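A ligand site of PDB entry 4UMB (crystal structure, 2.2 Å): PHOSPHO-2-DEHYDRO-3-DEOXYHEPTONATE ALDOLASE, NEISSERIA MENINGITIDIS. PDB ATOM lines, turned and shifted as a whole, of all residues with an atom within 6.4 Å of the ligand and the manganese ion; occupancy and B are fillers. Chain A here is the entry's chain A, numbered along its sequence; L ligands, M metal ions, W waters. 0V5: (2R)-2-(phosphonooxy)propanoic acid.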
ATOM      1  N   PRO A  62       3.158   1.174 -25.882  1.00  0.00           N
ATOM      2  CA  PRO A  62       2.361   0.696 -24.769  1.00  0.00           C
ATOM      3  C   PRO A  62       3.151  -0.044 -23.709  1.00  0.00           C
ATOM      4  O   PRO A  62       4.158  -0.703 -24.020  1.00  0.00           O
ATOM      5  CB  PRO A  62       1.416  -0.289 -25.455  1.00  0.00           C
ATOM      6  CG  PRO A  62       1.222   0.284 -26.829  1.00  0.00           C
ATOM      7  CD  PRO A  62       2.587   0.787 -27.183  1.00  0.00           C
ATOM      8  N   CYS A  63       2.661   0.011 -22.478  1.00  0.00           N
ATOM      9  CA  CYS A  63       3.203  -0.853 -21.446  1.00  0.00           C
ATOM     10  C   CYS A  63       3.138  -2.314 -21.912  1.00  0.00           C
ATOM     11  O   CYS A  63       4.120  -3.069 -21.812  1.00  0.00           O
ATOM     12  CB  CYS A  63       2.460  -0.679 -20.118  1.00  0.00           C
ATOM     13  SG  CYS A  63       3.004  -1.862 -18.854  1.00  0.00           S
ATOM     14  N   SER A  64       1.973  -2.689 -22.448  1.00  0.00           N
ATOM     15  CA  SER A  64       1.736  -4.043 -22.960  1.00  0.00           C
ATOM     16  C   SER A  64       0.862  -4.008 -24.186  1.00  0.00           C
ATOM     17  O   SER A  64      -0.011  -3.134 -24.312  1.00  0.00           O
ATOM     18  CB  SER A  64       1.050  -4.883 -21.905  1.00  0.00           C
ATOM     19  OG  SER A  64      -0.178  -4.283 -21.496  1.00  0.00           O
ATOM     20  N   ARG A  94       7.692  -0.002 -28.433  1.00  0.00           N
ATOM     21  CA  ARG A  94       7.450  -1.020 -27.380  1.00  0.00           C
ATOM     22  C   ARG A  94       6.367  -1.976 -27.817  1.00  0.00           C
ATOM     23  O   ARG A  94       5.213  -1.542 -28.079  1.00  0.00           O
ATOM     24  CB  ARG A  94       6.971  -0.369 -26.068  1.00  0.00           C
ATOM     25  CG  ARG A  94       8.033   0.387 -25.265  1.00  0.00           C
ATOM     26  CD  ARG A  94       7.479   0.983 -23.967  1.00  0.00           C
ATOM     27  NE  ARG A  94       6.825  -0.008 -23.122  1.00  0.00           N
ATOM     28  CZ  ARG A  94       7.325  -0.537 -21.996  1.00  0.00           C
ATOM     29  NH1 ARG A  94       8.471  -0.121 -21.470  1.00  0.00           N
ATOM     30  NH2 ARG A  94       6.647  -1.495 -21.361  1.00  0.00           N
ATOM     31  N   TYR A  96       5.582  -5.178 -26.182  1.00  0.00           N
ATOM     32  CA  TYR A  96       5.793  -6.091 -25.067  1.00  0.00           C
ATOM     33  C   TYR A  96       4.700  -7.168 -24.968  1.00  0.00           C
ATOM     34  O   TYR A  96       3.512  -6.862 -24.801  1.00  0.00           O
ATOM     35  CB  TYR A  96       5.848  -5.282 -23.756  1.00  0.00           C
ATOM     36  CG  TYR A  96       7.180  -4.605 -23.470  1.00  0.00           C
ATOM     37  CD1 TYR A  96       7.837  -3.831 -24.427  1.00  0.00           C
ATOM     38  CD2 TYR A  96       7.756  -4.689 -22.192  1.00  0.00           C
ATOM     39  CE1 TYR A  96       9.038  -3.191 -24.137  1.00  0.00           C
ATOM     40  CE2 TYR A  96       8.960  -4.052 -21.889  1.00  0.00           C
ATOM     41  CZ  TYR A  96       9.587  -3.318 -22.846  1.00  0.00           C
ATOM     42  OH  TYR A  96      10.759  -2.707 -22.547  1.00  0.00           O
ATOM     43  N   GLU A  98       5.166  -9.985 -22.810  1.00  0.00           N
ATOM     44  CA  GLU A  98       5.397 -10.724 -21.561  1.00  0.00           C
ATOM     45  C   GLU A  98       5.560  -9.746 -20.393  1.00  0.00           C
ATOM     46  O   GLU A  98       6.426  -8.885 -20.418  1.00  0.00           O
ATOM     47  CB  GLU A  98       6.652 -11.588 -21.710  1.00  0.00           C
ATOM     48  CG  GLU A  98       6.558 -12.607 -22.838  1.00  0.00           C
ATOM     49  CD  GLU A  98       7.858 -13.339 -23.143  1.00  0.00           C
ATOM     50  OE1 GLU A  98       8.878 -13.130 -22.448  1.00  0.00           O
ATOM     51  OE2 GLU A  98       7.851 -14.149 -24.087  1.00  0.00           O
ATOM     52  N   LYS A  99       4.696  -9.857 -19.397  1.00  0.00           N
ATOM     53  CA  LYS A  99       4.666  -8.919 -18.283  1.00  0.00           C
ATOM     54  C   LYS A  99       4.954  -9.627 -16.953  1.00  0.00           C
ATOM     55  O   LYS A  99       4.306 -10.607 -16.613  1.00  0.00           O
ATOM     56  CB  LYS A  99       3.321  -8.239 -18.193  1.00  0.00           C
ATOM     57  CG  LYS A  99       2.887  -7.545 -19.465  1.00  0.00           C
ATOM     58  CD  LYS A  99       3.913  -6.552 -20.004  1.00  0.00           C
ATOM     59  CE  LYS A  99       4.114  -5.388 -19.067  1.00  0.00           C
ATOM     60  NZ  LYS A  99       5.185  -4.468 -19.565  1.00  0.00           N
ATOM     61  N   PRO A 100       5.942  -9.129 -16.213  1.00  0.00           N
ATOM     62  CA  PRO A 100       6.245  -9.685 -14.901  1.00  0.00           C
ATOM     63  C   PRO A 100       5.375  -8.996 -13.882  1.00  0.00           C
ATOM     64  O   PRO A 100       5.408  -7.786 -13.778  1.00  0.00           O
ATOM     65  CB  PRO A 100       7.727  -9.349 -14.708  1.00  0.00           C
ATOM     66  CG  PRO A 100       7.905  -8.044 -15.448  1.00  0.00           C
ATOM     67  CD  PRO A 100       6.894  -8.055 -16.582  1.00  0.00           C
ATOM     68  N   GLU A 145      10.325  -6.921 -23.701  1.00  0.00           N
ATOM     69  CA  GLU A 145      11.043  -7.541 -22.583  1.00  0.00           C
ATOM     70  C   GLU A 145      11.081  -9.020 -22.856  1.00  0.00           C
ATOM     71  O   GLU A 145      10.048  -9.662 -23.101  1.00  0.00           O
ATOM     72  CB  GLU A 145      10.385  -7.270 -21.205  1.00  0.00           C
ATOM     73  CG  GLU A 145      10.997  -8.138 -20.088  1.00  0.00           C
ATOM     74  CD  GLU A 145      10.490  -7.869 -18.683  1.00  0.00           C
ATOM     75  OE1 GLU A 145       9.783  -6.835 -18.477  1.00  0.00           O
ATOM     76  OE2 GLU A 145      10.802  -8.682 -17.805  1.00  0.00           O
ATOM     77  N   ILE A 164      15.808  -6.726 -20.392  1.00  0.00           N
ATOM     78  CA  ILE A 164      15.674  -7.625 -19.253  1.00  0.00           C
ATOM     79  C   ILE A 164      15.188  -6.766 -18.097  1.00  0.00           C
ATOM     80  O   ILE A 164      15.807  -5.781 -17.744  1.00  0.00           O
ATOM     81  CB  ILE A 164      17.003  -8.322 -18.873  1.00  0.00           C
ATOM     82  CG1 ILE A 164      17.529  -9.123 -20.064  1.00  0.00           C
ATOM     83  CG2 ILE A 164      16.833  -9.194 -17.645  1.00  0.00           C
ATOM     84  CD1 ILE A 164      16.651 -10.275 -20.527  1.00  0.00           C
ATOM     85  N   GLY A 165      14.086  -7.159 -17.492  1.00  0.00           N
ATOM     86  CA  GLY A 165      13.399  -6.321 -16.534  1.00  0.00           C
ATOM     87  C   GLY A 165      14.130  -6.145 -15.206  1.00  0.00           C
ATOM     88  O   GLY A 165      15.014  -6.915 -14.838  1.00  0.00           O
ATOM     89  N   ALA A 166      13.695  -5.134 -14.457  1.00  0.00           N
ATOM     90  CA  ALA A 166      14.228  -4.870 -13.134  1.00  0.00           C
ATOM     91  C   ALA A 166      14.178  -6.110 -12.227  1.00  0.00           C
ATOM     92  O   ALA A 166      15.052  -6.295 -11.381  1.00  0.00           O
ATOM     93  CB  ALA A 166      13.463  -3.718 -12.494  1.00  0.00           C
ATOM     94  N   ARG A 167      13.136  -6.923 -12.400  1.00  0.00           N
ATOM     95  CA  ARG A 167      12.889  -8.075 -11.521  1.00  0.00           C
ATOM     96  C   ARG A 167      13.687  -9.329 -11.869  1.00  0.00           C
ATOM     97  O   ARG A 167      13.713 -10.287 -11.096  1.00  0.00           O
ATOM     98  CB  ARG A 167      11.386  -8.408 -11.499  1.00  0.00           C
ATOM     99  CG  ARG A 167      10.548  -7.313 -10.838  1.00  0.00           C
ATOM    100  CD  ARG A 167       9.037  -7.526 -11.013  1.00  0.00           C
ATOM    101  NE  ARG A 167       8.299  -6.304 -10.664  1.00  0.00           N
ATOM    102  CZ  ARG A 167       8.298  -5.189 -11.397  1.00  0.00           C
ATOM    103  NH1 ARG A 167       8.929  -5.088 -12.551  1.00  0.00           N
ATOM    104  NH2 ARG A 167       7.660  -4.122 -10.927  1.00  0.00           N
ATOM    105  N   LYS A 188      17.842  -3.479 -16.728  1.00  0.00           N
ATOM    106  CA  LYS A 188      17.337  -2.477 -15.814  1.00  0.00           C
ATOM    107  C   LYS A 188      17.916  -2.652 -14.406  1.00  0.00           C
ATOM    108  O   LYS A 188      18.170  -3.771 -13.962  1.00  0.00           O
ATOM    109  CB  LYS A 188      15.818  -2.559 -15.775  1.00  0.00           C
ATOM    110  CG  LYS A 188      15.166  -2.214 -17.129  1.00  0.00           C
ATOM    111  CD  LYS A 188      13.660  -2.053 -17.014  1.00  0.00           C
ATOM    112  CE  LYS A 188      13.127  -0.933 -17.884  1.00  0.00           C
ATOM    113  NZ  LYS A 188      11.741  -0.576 -17.477  1.00  0.00           N
ATOM    114  N   ASN A 189      18.114  -1.522 -13.729  1.00  0.00           N
ATOM    115  CA  ASN A 189      18.429  -1.557 -12.314  1.00  0.00           C
ATOM    116  C   ASN A 189      17.289  -2.249 -11.565  1.00  0.00           C
ATOM    117  O   ASN A 189      16.153  -2.344 -12.074  1.00  0.00           O
ATOM    118  CB  ASN A 189      18.747  -0.140 -11.765  1.00  0.00           C
ATOM    119  CG  ASN A 189      17.549   0.832 -11.773  1.00  0.00           C
ATOM    120  OD1 ASN A 189      17.547   1.821 -12.524  1.00  0.00           O
ATOM    121  ND2 ASN A 189      16.586   0.621 -10.876  1.00  0.00           N
ATOM    122  N   THR A 191      14.394  -3.181  -8.584  1.00  0.00           N
ATOM    123  CA  THR A 191      13.198  -2.415  -8.225  1.00  0.00           C
ATOM    124  C   THR A 191      13.422  -1.483  -7.029  1.00  0.00           C
ATOM    125  O   THR A 191      12.708  -0.481  -6.894  1.00  0.00           O
ATOM    126  CB  THR A 191      11.972  -3.340  -8.000  1.00  0.00           C
ATOM    127  OG1 THR A 191      12.314  -4.340  -7.042  1.00  0.00           O
ATOM    128  CG2 THR A 191      11.575  -3.999  -9.282  1.00  0.00           C
ATOM    129  N   ARG A 236      15.756   3.132 -14.319  1.00  0.00           N
ATOM    130  CA  ARG A 236      14.285   3.127 -14.284  1.00  0.00           C
ATOM    131  C   ARG A 236      13.739   3.426 -12.892  1.00  0.00           C
ATOM    132  O   ARG A 236      12.571   3.149 -12.595  1.00  0.00           O
ATOM    133  CB  ARG A 236      13.713   1.791 -14.825  1.00  0.00           C
ATOM    134  CG  ARG A 236      14.343   0.547 -14.213  1.00  0.00           C
ATOM    135  CD  ARG A 236      13.816   0.238 -12.830  1.00  0.00           C
ATOM    136  NE  ARG A 236      12.443  -0.257 -12.897  1.00  0.00           N
ATOM    137  CZ  ARG A 236      11.640  -0.339 -11.852  1.00  0.00           C
ATOM    138  NH1 ARG A 236      12.041   0.090 -10.655  1.00  0.00           N
ATOM    139  NH2 ARG A 236      10.432  -0.848 -11.994  1.00  0.00           N
ATOM    140  N   ASP A 267      14.691   5.398 -18.377  1.00  0.00           N
ATOM    141  CA  ASP A 267      13.274   5.138 -18.489  1.00  0.00           C
ATOM    142  C   ASP A 267      12.546   6.325 -17.845  1.00  0.00           C
ATOM    143  O   ASP A 267      12.769   6.639 -16.685  1.00  0.00           O
ATOM    144  CB  ASP A 267      12.947   3.809 -17.789  1.00  0.00           C
ATOM    145  CG  ASP A 267      11.482   3.384 -17.915  1.00  0.00           C
ATOM    146  OD1 ASP A 267      10.649   4.116 -18.497  1.00  0.00           O
ATOM    147  OD2 ASP A 267      11.177   2.279 -17.421  1.00  0.00           O
ATOM    148  N   SER A 269       9.351   6.268 -17.302  1.00  0.00           N
ATOM    149  CA  SER A 269       8.198   5.712 -16.612  1.00  0.00           C
ATOM    150  C   SER A 269       8.609   4.885 -15.353  1.00  0.00           C
ATOM    151  O   SER A 269       9.685   5.115 -14.764  1.00  0.00           O
ATOM    152  CB  SER A 269       7.362   4.859 -17.597  1.00  0.00           C
ATOM    153  OG  SER A 269       6.015   4.732 -17.172  1.00  0.00           O
ATOM    154  N   HIS A 270       7.705   4.014 -14.925  1.00  0.00           N
ATOM    155  CA  HIS A 270       7.880   3.179 -13.771  1.00  0.00           C
ATOM    156  C   HIS A 270       8.343   4.003 -12.569  1.00  0.00           C
ATOM    157  O   HIS A 270       7.667   4.962 -12.215  1.00  0.00           O
ATOM    158  CB  HIS A 270       8.743   2.001 -14.173  1.00  0.00           C
ATOM    159  CG  HIS A 270       8.210   1.320 -15.379  1.00  0.00           C
ATOM    160  ND1 HIS A 270       8.775   1.473 -16.632  1.00  0.00           N
ATOM    161  CD2 HIS A 270       7.082   0.586 -15.566  1.00  0.00           C
ATOM    162  CE1 HIS A 270       8.043   0.829 -17.527  1.00  0.00           C
ATOM    163  NE2 HIS A 270       7.010   0.283 -16.904  1.00  0.00           N
ATOM    164  N   ALA A 271       9.458   3.646 -11.931  1.00  0.00           N
ATOM    165  CA  ALA A 271       9.817   4.285 -10.658  1.00  0.00           C
ATOM    166  C   ALA A 271      10.415   5.655 -10.869  1.00  0.00           C
ATOM    167  O   ALA A 271      10.529   6.420  -9.924  1.00  0.00           O
ATOM    168  CB  ALA A 271      10.760   3.404  -9.852  1.00  0.00           C
ATOM    169  N   MET A 302      13.267   5.632 -22.599  1.00  0.00           N
ATOM    170  CA  MET A 302      12.131   4.741 -22.696  1.00  0.00           C
ATOM    171  C   MET A 302      10.897   5.523 -22.256  1.00  0.00           C
ATOM    172  O   MET A 302      10.982   6.361 -21.356  1.00  0.00           O
ATOM    173  CB  MET A 302      12.371   3.504 -21.841  1.00  0.00           C
ATOM    174  CG  MET A 302      11.310   2.416 -21.915  1.00  0.00           C
ATOM    175  SD  MET A 302      11.813   0.877 -21.063  1.00  0.00           S
ATOM    176  CE  MET A 302      13.581   1.144 -21.002  1.00  0.00           C
ATOM    177  N   GLU A 304       6.374   5.125 -21.865  1.00  0.00           N
ATOM    178  CA  GLU A 304       5.139   4.398 -21.941  1.00  0.00           C
ATOM    179  C   GLU A 304       4.019   5.299 -22.511  1.00  0.00           C
ATOM    180  O   GLU A 304       3.517   6.186 -21.830  1.00  0.00           O
ATOM    181  CB  GLU A 304       4.772   3.814 -20.566  1.00  0.00           C
ATOM    182  CG  GLU A 304       5.699   2.646 -20.194  1.00  0.00           C
ATOM    183  CD  GLU A 304       5.242   1.818 -19.017  1.00  0.00           C
ATOM    184  OE1 GLU A 304       4.914   2.354 -17.945  1.00  0.00           O
ATOM    185  OE2 GLU A 304       5.251   0.588 -19.187  1.00  0.00           O
ATOM    186  N   THR A 323      -2.396  -2.404 -18.460  1.00  0.00           N
ATOM    187  CA  THR A 323      -1.324  -2.579 -17.447  1.00  0.00           C
ATOM    188  C   THR A 323      -0.937  -1.176 -16.934  1.00  0.00           C
ATOM    189  O   THR A 323      -1.838  -0.422 -16.519  1.00  0.00           O
ATOM    190  CB  THR A 323      -0.167  -3.427 -17.999  1.00  0.00           C
ATOM    191  OG1 THR A 323       0.222  -2.975 -19.302  1.00  0.00           O
ATOM    192  CG2 THR A 323      -0.602  -4.896 -18.118  1.00  0.00           C
ATOM    193  N   ASP A 324       0.349  -0.802 -16.965  1.00  0.00           N
ATOM    194  CA  ASP A 324       0.726   0.507 -16.417  1.00  0.00           C
ATOM    195  C   ASP A 324       0.045   1.603 -17.239  1.00  0.00           C
ATOM    196  O   ASP A 324      -0.127   1.464 -18.443  1.00  0.00           O
ATOM    197  CB  ASP A 324       2.232   0.763 -16.469  1.00  0.00           C
ATOM    198  CG  ASP A 324       3.045  -0.258 -15.695  1.00  0.00           C
ATOM    199  OD1 ASP A 324       2.513  -0.787 -14.706  1.00  0.00           O
ATOM    200  OD2 ASP A 324       4.203  -0.515 -16.091  1.00  0.00           O
HETATM  201  C1  0V5 L   1       7.536  -2.360 -18.082  1.00  0.00           C
HETATM  202  O1  0V5 L   1       6.288  -2.347 -18.131  1.00  0.00           O
HETATM  203  O2' 0V5 L   1       8.316  -2.034 -18.998  1.00  0.00           O
HETATM  204  C2  0V5 L   1       8.120  -2.866 -16.773  1.00  0.00           C
HETATM  205  C3  0V5 L   1       7.945  -4.385 -16.806  1.00  0.00           C
HETATM  206  O2  0V5 L   1       9.507  -2.521 -16.643  1.00  0.00           O
HETATM  207  P   0V5 L   1      10.225  -2.639 -15.185  1.00  0.00           P
HETATM  208  O1P 0V5 L   1      11.116  -3.954 -15.354  1.00  0.00           O
HETATM  209  O2P 0V5 L   1      11.292  -1.442 -15.097  1.00  0.00           O
HETATM  210  O3P 0V5 L   1       9.252  -2.831 -14.051  1.00  0.00           O
HETATM  211 MN    MN M   1       5.069  -0.781 -17.700  1.00  0.00          MN
HETATM  212  O   HOH W   1      11.255  -4.500 -18.135  1.00  0.00           O
HETATM  213  O   HOH W   2      10.766  -6.403 -14.110  1.00  0.00           O
HETATM  214  O   HOH W   3       7.304  -6.362 -19.432  1.00  0.00           O
HETATM  215  O   HOH W   4      10.860  -2.459 -19.836  1.00  0.00           O
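Water W4 lies within hydrogen-bond range of an oxygen (O2') of the ligand, the side-chain hydroxyl (OH) of Tyr 96, the side-chain amino group (NZ) of Lys 188 and the side-chain sulfur (SD) of Met 302. Water W2 lies within hydrogen-bond range of the guanidinium group (NH1) of Arg 167 (2.7 Å), an oxygen (O1P) of the ligand (2.8 Å) and the backbone NH (N) of Ala 166 (3.2 Å). Water W1 bridges the side-chain carboxylate of Glu 145 (2.8 Å) and an oxygen (O1P) of the ligand (2.8 Å). Water W3 lies within hydrogen-bond range of OE1 of Glu 145 (2.7 Å), NZ of Lys 99 (2.8 Å) and O of Glu 98 (2.8 Å).
The manganese ion is bound by the side-chain carboxylate of Asp 324 (1.8 Å), the side-chain carboxylate of Glu 304 (2.0 Å), an oxygen (O1) of the ligand (2.0 Å), a ring nitrogen (NE2) of His 270 (2.4 Å) and the side-chain sulfur of Cys 63 (2.6 Å). The manganese ion has five donor atoms within binding distance.
Within 4 Å of the manganese ion: Cys 63, His 270, Glu 304 and Asp 324.
Tyr 96 touches the ligand. CD of Pro 100 touches C3 of the ligand, 3.8 Å away. OE1 of Glu 145 touches C3 of the ligand, 3.5 Å away. CA of Gly 165 touches O1P of the ligand, 3.5 Å away. Hydrophobic or aromatic side chains that line the ligand: Tyr 96, Pro 100, Ala 166 and His 270. 14 residues have an atom within 4 Å of the ligand: Cys 63, Arg 94, Tyr 96, Lys 99, Pro 100, Glu 145, Gly 165, Ala 166, Arg 167, Lys 188, Arg 236, His 270, Glu 304 and Asp 324.
OE2 of Glu 304 sits close to NH2 of Arg 94, 3.3 Å away. A ring nitrogen (ND1) of His 270 sits at hydrogen-bond distance from the side-chain carboxylate of Asp 267 (2.7 Å). The side-chain amino group (NZ) of Lys 188 lies within salt-bridge range of the side-chain carboxylate (OD2) of Asp 267, at 2.9 Å. The side-chain amino group of Lys 99 sits at hydrogen-bond distance from the backbone carbonyl oxygen of Cys 63 (2.9 Å). The backbone carbonyl oxygen of Cys 63 lies within hydrogen-bond range of the guanidinium group of Arg 94 (3.0 Å). SG of Cys 63 sits close to OG1 of Thr 323 (3.0 Å). The guanidinium group (NH1) of Arg 94 lies within hydrogen-bond range of the side-chain sulfur (SD) of Met 302 (3.5 Å). NE of Arg 94 is in hydrogen-bond range of O of Pro 62, 2.9 Å away.
An oxygen (O2P) of the ligand lies within salt-bridge range of the side-chain amino group (NZ) of Lys 188, 2.6 Å away. NH1 of Arg 167 is in salt-bridge range of O3P of the ligand, at 2.7 Å. O2P of the ligand is in salt-bridge range of NE of Arg 236, 2.8 Å away. An oxygen (O1) of the ligand lies close to the side-chain amino group (NZ) of Lys 99, at 2.8 Å. The guanidinium group (NH2) of Arg 94 is in salt-bridge range of an oxygen (O2') of the ligand (2.9 Å). The backbone NH (N) of Ala 166 is in hydrogen-bond range of an oxygen (O1P) of the ligand, at 3.0 Å.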
